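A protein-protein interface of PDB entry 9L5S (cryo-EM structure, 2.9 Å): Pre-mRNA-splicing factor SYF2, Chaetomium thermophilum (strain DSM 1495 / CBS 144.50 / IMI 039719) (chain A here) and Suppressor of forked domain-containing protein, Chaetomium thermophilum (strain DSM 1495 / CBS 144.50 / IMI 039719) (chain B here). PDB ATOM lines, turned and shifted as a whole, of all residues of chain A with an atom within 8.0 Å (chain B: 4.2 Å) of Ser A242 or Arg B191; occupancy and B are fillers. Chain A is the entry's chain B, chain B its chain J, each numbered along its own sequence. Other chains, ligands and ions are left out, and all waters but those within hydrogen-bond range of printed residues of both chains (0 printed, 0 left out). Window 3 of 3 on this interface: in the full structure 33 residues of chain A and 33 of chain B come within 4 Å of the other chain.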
ATOM      1  N   TYR A 204     -36.295 -12.233  -8.551  1.00  0.00           N
ATOM      2  CA  TYR A 204     -35.235 -11.345  -9.028  1.00  0.00           C
ATOM      3  C   TYR A 204     -34.489 -11.954 -10.210  1.00  0.00           C
ATOM      4  O   TYR A 204     -34.060 -11.237 -11.122  1.00  0.00           O
ATOM      5  CB  TYR A 204     -34.276 -11.039  -7.875  1.00  0.00           C
ATOM      6  CG  TYR A 204     -33.112 -10.135  -8.215  1.00  0.00           C
ATOM      7  CD1 TYR A 204     -33.295  -8.771  -8.408  1.00  0.00           C
ATOM      8  CD2 TYR A 204     -31.825 -10.648  -8.331  1.00  0.00           C
ATOM      9  CE1 TYR A 204     -32.230  -7.943  -8.712  1.00  0.00           C
ATOM     10  CE2 TYR A 204     -30.756  -9.828  -8.636  1.00  0.00           C
ATOM     11  CZ  TYR A 204     -30.966  -8.478  -8.825  1.00  0.00           C
ATOM     12  OH  TYR A 204     -29.910  -7.653  -9.129  1.00  0.00           O
ATOM     13  N   LYS A 208     -34.421 -10.074 -13.758  1.00  0.00           N
ATOM     14  CA  LYS A 208     -33.106  -9.879 -14.369  1.00  0.00           C
ATOM     15  C   LYS A 208     -33.079 -10.429 -15.791  1.00  0.00           C
ATOM     16  O   LYS A 208     -32.600  -9.753 -16.707  1.00  0.00           O
ATOM     17  CB  LYS A 208     -32.010 -10.520 -13.518  1.00  0.00           C
ATOM     18  CG  LYS A 208     -30.604 -10.372 -14.104  1.00  0.00           C
ATOM     19  CD  LYS A 208     -29.549 -11.067 -13.253  1.00  0.00           C
ATOM     20  CE  LYS A 208     -29.140 -10.200 -12.072  1.00  0.00           C
ATOM     21  NZ  LYS A 208     -27.848 -10.650 -11.495  1.00  0.00           N
ATOM     22  N   ASP A 235     -22.785  -4.253 -20.686  1.00  0.00           N
ATOM     23  CA  ASP A 235     -23.632  -3.068 -20.662  1.00  0.00           C
ATOM     24  C   ASP A 235     -22.856  -1.892 -21.235  1.00  0.00           C
ATOM     25  O   ASP A 235     -21.758  -1.583 -20.761  1.00  0.00           O
ATOM     26  CB  ASP A 235     -24.100  -2.762 -19.238  1.00  0.00           C
ATOM     27  CG  ASP A 235     -25.320  -1.865 -19.206  1.00  0.00           C
ATOM     28  OD1 ASP A 235     -25.818  -1.489 -20.288  1.00  0.00           O
ATOM     29  OD2 ASP A 235     -25.765  -1.515 -18.095  1.00  0.00           O
ATOM     30  N   ASP A 237     -24.025   1.365 -21.240  1.00  0.00           N
ATOM     31  CA  ASP A 237     -24.219   2.391 -20.229  1.00  0.00           C
ATOM     32  C   ASP A 237     -24.142   1.762 -18.838  1.00  0.00           C
ATOM     33  O   ASP A 237     -23.657   0.641 -18.662  1.00  0.00           O
ATOM     34  CB  ASP A 237     -25.546   3.109 -20.461  1.00  0.00           C
ATOM     35  CG  ASP A 237     -25.527   3.981 -21.701  1.00  0.00           C
ATOM     36  OD1 ASP A 237     -24.504   4.658 -21.937  1.00  0.00           O
ATOM     37  OD2 ASP A 237     -26.534   3.989 -22.439  1.00  0.00           O
ATOM     38  N   GLY A 238     -24.589   2.501 -17.826  1.00  0.00           N
ATOM     39  CA  GLY A 238     -24.727   1.954 -16.491  1.00  0.00           C
ATOM     40  C   GLY A 238     -26.175   1.888 -16.049  1.00  0.00           C
ATOM     41  O   GLY A 238     -26.466   1.803 -14.852  1.00  0.00           O
ATOM     42  N   THR A 239     -27.093   1.929 -17.013  1.00  0.00           N
ATOM     43  CA  THR A 239     -28.523   2.014 -16.744  1.00  0.00           C
ATOM     44  C   THR A 239     -29.136   0.710 -16.246  1.00  0.00           C
ATOM     45  O   THR A 239     -30.244   0.734 -15.701  1.00  0.00           O
ATOM     46  CB  THR A 239     -29.263   2.470 -18.005  1.00  0.00           C
ATOM     47  OG1 THR A 239     -29.204   1.439 -18.998  1.00  0.00           O
ATOM     48  CG2 THR A 239     -28.642   3.740 -18.556  1.00  0.00           C
ATOM     49  N   PHE A 240     -28.453  -0.424 -16.414  1.00  0.00           N
ATOM     50  CA  PHE A 240     -29.023  -1.705 -16.007  1.00  0.00           C
ATOM     51  C   PHE A 240     -28.746  -2.003 -14.537  1.00  0.00           C
ATOM     52  O   PHE A 240     -29.633  -2.469 -13.811  1.00  0.00           O
ATOM     53  CB  PHE A 240     -28.480  -2.827 -16.897  1.00  0.00           C
ATOM     54  CG  PHE A 240     -29.004  -4.192 -16.548  1.00  0.00           C
ATOM     55  CD1 PHE A 240     -30.260  -4.592 -16.966  1.00  0.00           C
ATOM     56  CD2 PHE A 240     -28.228  -5.083 -15.819  1.00  0.00           C
ATOM     57  CE1 PHE A 240     -30.741  -5.848 -16.650  1.00  0.00           C
ATOM     58  CE2 PHE A 240     -28.706  -6.340 -15.501  1.00  0.00           C
ATOM     59  CZ  PHE A 240     -29.964  -6.722 -15.918  1.00  0.00           C
ATOM     60  N   PHE A 241     -27.506  -1.768 -14.095  1.00  0.00           N
ATOM     61  CA  PHE A 241     -27.102  -2.103 -12.731  1.00  0.00           C
ATOM     62  C   PHE A 241     -27.879  -1.293 -11.700  1.00  0.00           C
ATOM     63  O   PHE A 241     -28.663  -1.841 -10.917  1.00  0.00           O
ATOM     64  CB  PHE A 241     -25.597  -1.875 -12.577  1.00  0.00           C
ATOM     65  CG  PHE A 241     -24.752  -2.932 -13.223  1.00  0.00           C
ATOM     66  CD1 PHE A 241     -25.308  -4.137 -13.619  1.00  0.00           C
ATOM     67  CD2 PHE A 241     -23.401  -2.718 -13.443  1.00  0.00           C
ATOM     68  CE1 PHE A 241     -24.535  -5.109 -14.211  1.00  0.00           C
ATOM     69  CE2 PHE A 241     -22.621  -3.689 -14.040  1.00  0.00           C
ATOM     70  CZ  PHE A 241     -23.191  -4.886 -14.424  1.00  0.00           C
ATOM     71  N   SER A 242     -27.671   0.017 -11.689  1.00  0.00           N
ATOM     72  CA  SER A 242     -28.484   0.945 -10.919  1.00  0.00           C
ATOM     73  C   SER A 242     -29.205   1.849 -11.905  1.00  0.00           C
ATOM     74  O   SER A 242     -28.623   2.246 -12.920  1.00  0.00           O
ATOM     75  CB  SER A 242     -27.631   1.768  -9.951  1.00  0.00           C
ATOM     76  OG  SER A 242     -26.743   2.623 -10.649  1.00  0.00           O
ATOM     77  N   THR A 243     -30.459   2.180 -11.613  1.00  0.00           N
ATOM     78  CA  THR A 243     -31.249   2.946 -12.570  1.00  0.00           C
ATOM     79  C   THR A 243     -30.915   4.440 -12.564  1.00  0.00           C
ATOM     80  O   THR A 243     -31.677   5.230 -13.130  1.00  0.00           O
ATOM     81  CB  THR A 243     -32.746   2.727 -12.330  1.00  0.00           C
ATOM     82  OG1 THR A 243     -33.498   3.487 -13.282  1.00  0.00           O
ATOM     83  CG2 THR A 243     -33.140   3.146 -10.934  1.00  0.00           C
ATOM     84  N   ALA A 244     -29.814   4.844 -11.932  1.00  0.00           N
ATOM     85  CA  ALA A 244     -29.175   6.102 -12.287  1.00  0.00           C
ATOM     86  C   ALA A 244     -28.650   5.999 -13.713  1.00  0.00           C
ATOM     87  O   ALA A 244     -28.258   4.916 -14.159  1.00  0.00           O
ATOM     88  CB  ALA A 244     -28.040   6.423 -11.315  1.00  0.00           C
ATOM     89  N   ASN A 245     -28.701   7.132 -14.435  1.00  0.00           N
ATOM     90  CA  ASN A 245     -28.502   7.293 -15.882  1.00  0.00           C
ATOM     91  C   ASN A 245     -29.646   6.685 -16.689  1.00  0.00           C
ATOM     92  O   ASN A 245     -29.679   6.812 -17.918  1.00  0.00           O
ATOM     93  CB  ASN A 245     -27.169   6.707 -16.369  1.00  0.00           C
ATOM     94  CG  ASN A 245     -26.052   7.718 -16.367  1.00  0.00           C
ATOM     95  OD1 ASN A 245     -26.221   8.847 -16.826  1.00  0.00           O
ATOM     96  ND2 ASN A 245     -24.894   7.315 -15.859  1.00  0.00           N
ATOM     97  N   ALA A 246     -30.589   6.039 -16.014  1.00  0.00           N
ATOM     98  CA  ALA A 246     -31.793   5.507 -16.634  1.00  0.00           C
ATOM     99  C   ALA A 246     -32.946   6.415 -16.235  1.00  0.00           C
ATOM    100  O   ALA A 246     -33.446   6.336 -15.109  1.00  0.00           O
ATOM    101  CB  ALA A 246     -32.047   4.065 -16.204  1.00  0.00           C
ATOM    102  N   PHE A 249     -36.585   5.487 -14.487  1.00  0.00           N
ATOM    103  CA  PHE A 249     -36.811   5.068 -13.110  1.00  0.00           C
ATOM    104  C   PHE A 249     -38.180   5.510 -12.615  1.00  0.00           C
ATOM    105  O   PHE A 249     -38.722   4.896 -11.691  1.00  0.00           O
ATOM    106  CB  PHE A 249     -35.707   5.610 -12.191  1.00  0.00           C
ATOM    107  CG  PHE A 249     -35.727   7.108 -12.007  1.00  0.00           C
ATOM    108  CD1 PHE A 249     -35.151   7.947 -12.950  1.00  0.00           C
ATOM    109  CD2 PHE A 249     -36.289   7.674 -10.871  1.00  0.00           C
ATOM    110  CE1 PHE A 249     -35.160   9.317 -12.779  1.00  0.00           C
ATOM    111  CE2 PHE A 249     -36.301   9.045 -10.696  1.00  0.00           C
ATOM    112  CZ  PHE A 249     -35.734   9.866 -11.650  1.00  0.00           C
ATOM    113  N   PRO B 157     -33.066  -2.068  -8.487  1.00  0.00           N
ATOM    114  CA  PRO B 157     -32.223  -0.969  -9.003  1.00  0.00           C
ATOM    115  C   PRO B 157     -32.572   0.406  -8.455  1.00  0.00           C
ATOM    116  O   PRO B 157     -31.670   1.241  -8.296  1.00  0.00           O
ATOM    117  CB  PRO B 157     -32.452  -1.040 -10.517  1.00  0.00           C
ATOM    118  CG  PRO B 157     -32.704  -2.454 -10.765  1.00  0.00           C
ATOM    119  CD  PRO B 157     -33.542  -2.905  -9.610  1.00  0.00           C
ATOM    120  N   ARG B 160     -30.964   0.564  -5.199  1.00  0.00           N
ATOM    121  CA  ARG B 160     -29.528   0.697  -5.417  1.00  0.00           C
ATOM    122  C   ARG B 160     -29.138   2.128  -5.768  1.00  0.00           C
ATOM    123  O   ARG B 160     -28.100   2.614  -5.314  1.00  0.00           O
ATOM    124  CB  ARG B 160     -29.069  -0.270  -6.505  1.00  0.00           C
ATOM    125  CG  ARG B 160     -28.687  -1.640  -5.972  1.00  0.00           C
ATOM    126  CD  ARG B 160     -28.030  -2.481  -7.044  1.00  0.00           C
ATOM    127  NE  ARG B 160     -28.374  -3.895  -6.952  1.00  0.00           N
ATOM    128  CZ  ARG B 160     -29.295  -4.491  -7.696  1.00  0.00           C
ATOM    129  NH1 ARG B 160     -29.989  -3.825  -8.602  1.00  0.00           N
ATOM    130  NH2 ARG B 160     -29.527  -5.790  -7.523  1.00  0.00           N
ATOM    131  N   ASP B 164     -26.893   4.691  -3.794  1.00  0.00           N
ATOM    132  CA  ASP B 164     -25.784   5.384  -4.444  1.00  0.00           C
ATOM    133  C   ASP B 164     -25.779   6.869  -4.102  1.00  0.00           C
ATOM    134  O   ASP B 164     -24.714   7.452  -3.872  1.00  0.00           O
ATOM    135  CB  ASP B 164     -25.851   5.182  -5.958  1.00  0.00           C
ATOM    136  CG  ASP B 164     -25.034   3.993  -6.424  1.00  0.00           C
ATOM    137  OD1 ASP B 164     -23.903   3.815  -5.925  1.00  0.00           O
ATOM    138  OD2 ASP B 164     -25.520   3.239  -7.293  1.00  0.00           O
ATOM    139  N   GLU B 183     -26.821  -5.777  -1.243  1.00  0.00           N
ATOM    140  CA  GLU B 183     -26.245  -6.432  -2.413  1.00  0.00           C
ATOM    141  C   GLU B 183     -25.885  -7.886  -2.140  1.00  0.00           C
ATOM    142  O   GLU B 183     -25.878  -8.695  -3.070  1.00  0.00           O
ATOM    143  CB  GLU B 183     -25.037  -5.653  -2.919  1.00  0.00           C
ATOM    144  CG  GLU B 183     -25.387  -4.258  -3.397  1.00  0.00           C
ATOM    145  CD  GLU B 183     -25.822  -4.228  -4.851  1.00  0.00           C
ATOM    146  OE1 GLU B 183     -26.833  -4.875  -5.193  1.00  0.00           O
ATOM    147  OE2 GLU B 183     -25.146  -3.557  -5.660  1.00  0.00           O
ATOM    148  N   GLU B 188     -25.047 -10.954  -6.099  1.00  0.00           N
ATOM    149  CA  GLU B 188     -24.389  -9.673  -6.419  1.00  0.00           C
ATOM    150  C   GLU B 188     -23.235  -9.326  -5.470  1.00  0.00           C
ATOM    151  O   GLU B 188     -23.280  -8.359  -4.709  1.00  0.00           O
ATOM    152  CB  GLU B 188     -25.420  -8.540  -6.451  1.00  0.00           C
ATOM    153  CG  GLU B 188     -26.433  -8.644  -7.586  1.00  0.00           C
ATOM    154  CD  GLU B 188     -25.996  -7.927  -8.851  1.00  0.00           C
ATOM    155  OE1 GLU B 188     -24.804  -8.010  -9.214  1.00  0.00           O
ATOM    156  OE2 GLU B 188     -26.854  -7.281  -9.488  1.00  0.00           O
ATOM    157  N   TYR B 189     -22.197 -10.154  -5.534  1.00  0.00           N
ATOM    158  CA  TYR B 189     -21.062 -10.024  -4.627  1.00  0.00           C
ATOM    159  C   TYR B 189     -19.983  -9.089  -5.156  1.00  0.00           C
ATOM    160  O   TYR B 189     -19.321  -8.402  -4.365  1.00  0.00           O
ATOM    161  CB  TYR B 189     -20.470 -11.408  -4.361  1.00  0.00           C
ATOM    162  CG  TYR B 189     -21.460 -12.342  -3.708  1.00  0.00           C
ATOM    163  CD1 TYR B 189     -21.982 -12.065  -2.451  1.00  0.00           C
ATOM    164  CD2 TYR B 189     -21.903 -13.480  -4.368  1.00  0.00           C
ATOM    165  CE1 TYR B 189     -22.897 -12.910  -1.860  1.00  0.00           C
ATOM    166  CE2 TYR B 189     -22.820 -14.328  -3.786  1.00  0.00           C
ATOM    167  CZ  TYR B 189     -23.311 -14.040  -2.532  1.00  0.00           C
ATOM    168  OH  TYR B 189     -24.224 -14.885  -1.949  1.00  0.00           O
ATOM    169  N   GLU B 190     -19.788  -9.049  -6.475  1.00  0.00           N
ATOM    170  CA  GLU B 190     -18.756  -8.194  -7.054  1.00  0.00           C
ATOM    171  C   GLU B 190     -19.101  -6.717  -6.890  1.00  0.00           C
ATOM    172  O   GLU B 190     -18.220  -5.885  -6.625  1.00  0.00           O
ATOM    173  CB  GLU B 190     -18.569  -8.547  -8.527  1.00  0.00           C
ATOM    174  CG  GLU B 190     -17.220  -8.164  -9.082  1.00  0.00           C
ATOM    175  CD  GLU B 190     -17.221  -6.788  -9.707  1.00  0.00           C
ATOM    176  OE1 GLU B 190     -18.310  -6.297 -10.072  1.00  0.00           O
ATOM    177  OE2 GLU B 190     -16.129  -6.198  -9.843  1.00  0.00           O
ATOM    178  N   ARG B 191     -20.382  -6.373  -7.022  1.00  0.00           N
ATOM    179  CA  ARG B 191     -20.779  -4.989  -6.806  1.00  0.00           C
ATOM    180  C   ARG B 191     -20.631  -4.612  -5.340  1.00  0.00           C
ATOM    181  O   ARG B 191     -20.259  -3.476  -5.024  1.00  0.00           O
ATOM    182  CB  ARG B 191     -22.206  -4.776  -7.295  1.00  0.00           C
ATOM    183  CG  ARG B 191     -22.315  -4.940  -8.796  1.00  0.00           C
ATOM    184  CD  ARG B 191     -23.723  -4.747  -9.287  1.00  0.00           C
ATOM    185  NE  ARG B 191     -24.149  -3.369  -9.100  1.00  0.00           N
ATOM    186  CZ  ARG B 191     -25.386  -2.936  -9.291  1.00  0.00           C
ATOM    187  NH1 ARG B 191     -26.364  -3.764  -9.614  1.00  0.00           N
ATOM    188  NH2 ARG B 191     -25.643  -1.637  -9.167  1.00  0.00           N
ATOM    189  N   ALA B 192     -20.851  -5.574  -4.440  1.00  0.00           N
ATOM    190  CA  ALA B 192     -20.497  -5.369  -3.044  1.00  0.00           C
ATOM    191  C   ALA B 192     -18.996  -5.176  -2.869  1.00  0.00           C
ATOM    192  O   ALA B 192     -18.573  -4.475  -1.948  1.00  0.00           O
ATOM    193  CB  ALA B 192     -20.987  -6.542  -2.196  1.00  0.00           C
ATOM    194  N   ARG B 193     -18.174  -5.769  -3.742  1.00  0.00           N
ATOM    195  CA  ARG B 193     -16.734  -5.517  -3.666  1.00  0.00           C
ATOM    196  C   ARG B 193     -16.395  -4.074  -4.040  1.00  0.00           C
ATOM    197  O   ARG B 193     -15.540  -3.450  -3.395  1.00  0.00           O
ATOM    198  CB  ARG B 193     -15.961  -6.499  -4.550  1.00  0.00           C
ATOM    199  CG  ARG B 193     -16.003  -7.938  -4.073  1.00  0.00           C
ATOM    200  CD  ARG B 193     -15.044  -8.816  -4.859  1.00  0.00           C
ATOM    201  NE  ARG B 193     -15.084 -10.200  -4.401  1.00  0.00           N
ATOM    202  CZ  ARG B 193     -15.832 -11.149  -4.947  1.00  0.00           C
ATOM    203  NH1 ARG B 193     -16.609 -10.904  -5.989  1.00  0.00           N
ATOM    204  NH2 ARG B 193     -15.799 -12.376  -4.434  1.00  0.00           N
ATOM    205  N   GLN B 194     -17.053  -3.515  -5.067  1.00  0.00           N
ATOM    206  CA  GLN B 194     -16.849  -2.076  -5.298  1.00  0.00           C
ATOM    207  C   GLN B 194     -17.399  -1.228  -4.149  1.00  0.00           C
ATOM    208  O   GLN B 194     -16.864  -0.146  -3.860  1.00  0.00           O
ATOM    209  CB  GLN B 194     -17.426  -1.555  -6.625  1.00  0.00           C
ATOM    210  CG  GLN B 194     -16.679  -1.928  -7.907  1.00  0.00           C
ATOM    211  CD  GLN B 194     -17.092  -3.232  -8.516  1.00  0.00           C
ATOM    212  OE1 GLN B 194     -18.174  -3.728  -8.247  1.00  0.00           O
ATOM    213  NE2 GLN B 194     -16.232  -3.797  -9.353  1.00  0.00           N
ATOM    214  N   ILE B 195     -18.465  -1.690  -3.488  1.00  0.00           N
ATOM    215  CA  ILE B 195     -18.965  -0.958  -2.322  1.00  0.00           C
ATOM    216  C   ILE B 195     -17.948  -0.983  -1.183  1.00  0.00           C
ATOM    217  O   ILE B 195     -17.753   0.024  -0.500  1.00  0.00           O
ATOM    218  CB  ILE B 195     -20.341  -1.488  -1.878  1.00  0.00           C
ATOM    219  CG1 ILE B 195     -21.355  -1.301  -2.994  1.00  0.00           C
ATOM    220  CG2 ILE B 195     -20.847  -0.735  -0.662  1.00  0.00           C
ATOM    221  CD1 ILE B 195     -22.585  -2.102  -2.794  1.00  0.00           C
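The guanidinium group (NH2) of Arg B160 sits at hydrogen-bond distance from the side-chain hydroxyl (OH) of Tyr A204, 2.5 Å away. NH1 of Arg B160 sits at hydrogen-bond distance from O of Phe A241, 3.3 Å away. OE2 of Glu B188 is in hydrogen-bond range of OH of Tyr A204, at 3.1 Å. NH1 of Arg B191 lies within hydrogen-bond range of O of Phe A241 (3.3 Å).
The guanidinium group of Arg B160 lies within salt-bridge range of the side-chain carboxylate of Glu B183, 2.5 Å away. NH2 of Arg B160 is in salt-bridge range of OE2 of Glu B188, 3.6 Å away. The guanidinium group of Arg B191 is in salt-bridge range of the side-chain carboxylate of Glu B183, at 3.6 Å. OE2 of Glu B188 lies within salt-bridge range of NH1 of Arg B191 (3.6 Å). The backbone carbonyl oxygen of Ala A246 sits close to the side-chain hydroxyl of Thr A243, at 3.4 Å.
Among the printed residues, pairs that only touch across the chains: Thr A243 with Pro B157, Ser A242 with Asp B164, Ser A242 with Arg B191 and Phe A241 with Pro B157.
Asp A235 touches none of the printed residues of chain B. Of the printed residues of chain B, Phe A241 touches Pro B157 (3.9 Å), Arg B160 (3.3 Å) and Arg B191 (3.3 Å). Of the printed residues of chain B, Ser A242 touches Asp B164 (3.6 Å) and Arg B191 (3.6 Å). Printed residues of chain B within 4 Å of Thr A243: Pro B157 (3.6 Å). Of the printed residues of chain A, Asp B164 touches Ser A242. Tyr B189 touches none of the printed residues of chain A. Arg B191 touches just these residues of chain A: Phe A241 and Ser A242. Ala B192 touches none of the printed residues of chain A. The nearest residue of chain B that does not touch Ser A242 is Pro B157 (4.1 Å). The nearest printed residue of chain B that does not touch Tyr A204 is Pro B157 (5.3 Å).
Along chain B the printed residues that touch a printed residue of chain A span positions 157 to 191. Printed residues of chain A that touch a printed residue of chain B: Tyr A204, Phe A241, Ser A242 and Thr A243. Hydrophobic or aromatic side chains of chain A within 4 Å of the printed part of chain B: Tyr A204 and Phe A241. Among the printed residues, no Asp or Glu carboxylate lies within 4 Å of a Lys or Arg side-chain nitrogen of the other chain.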
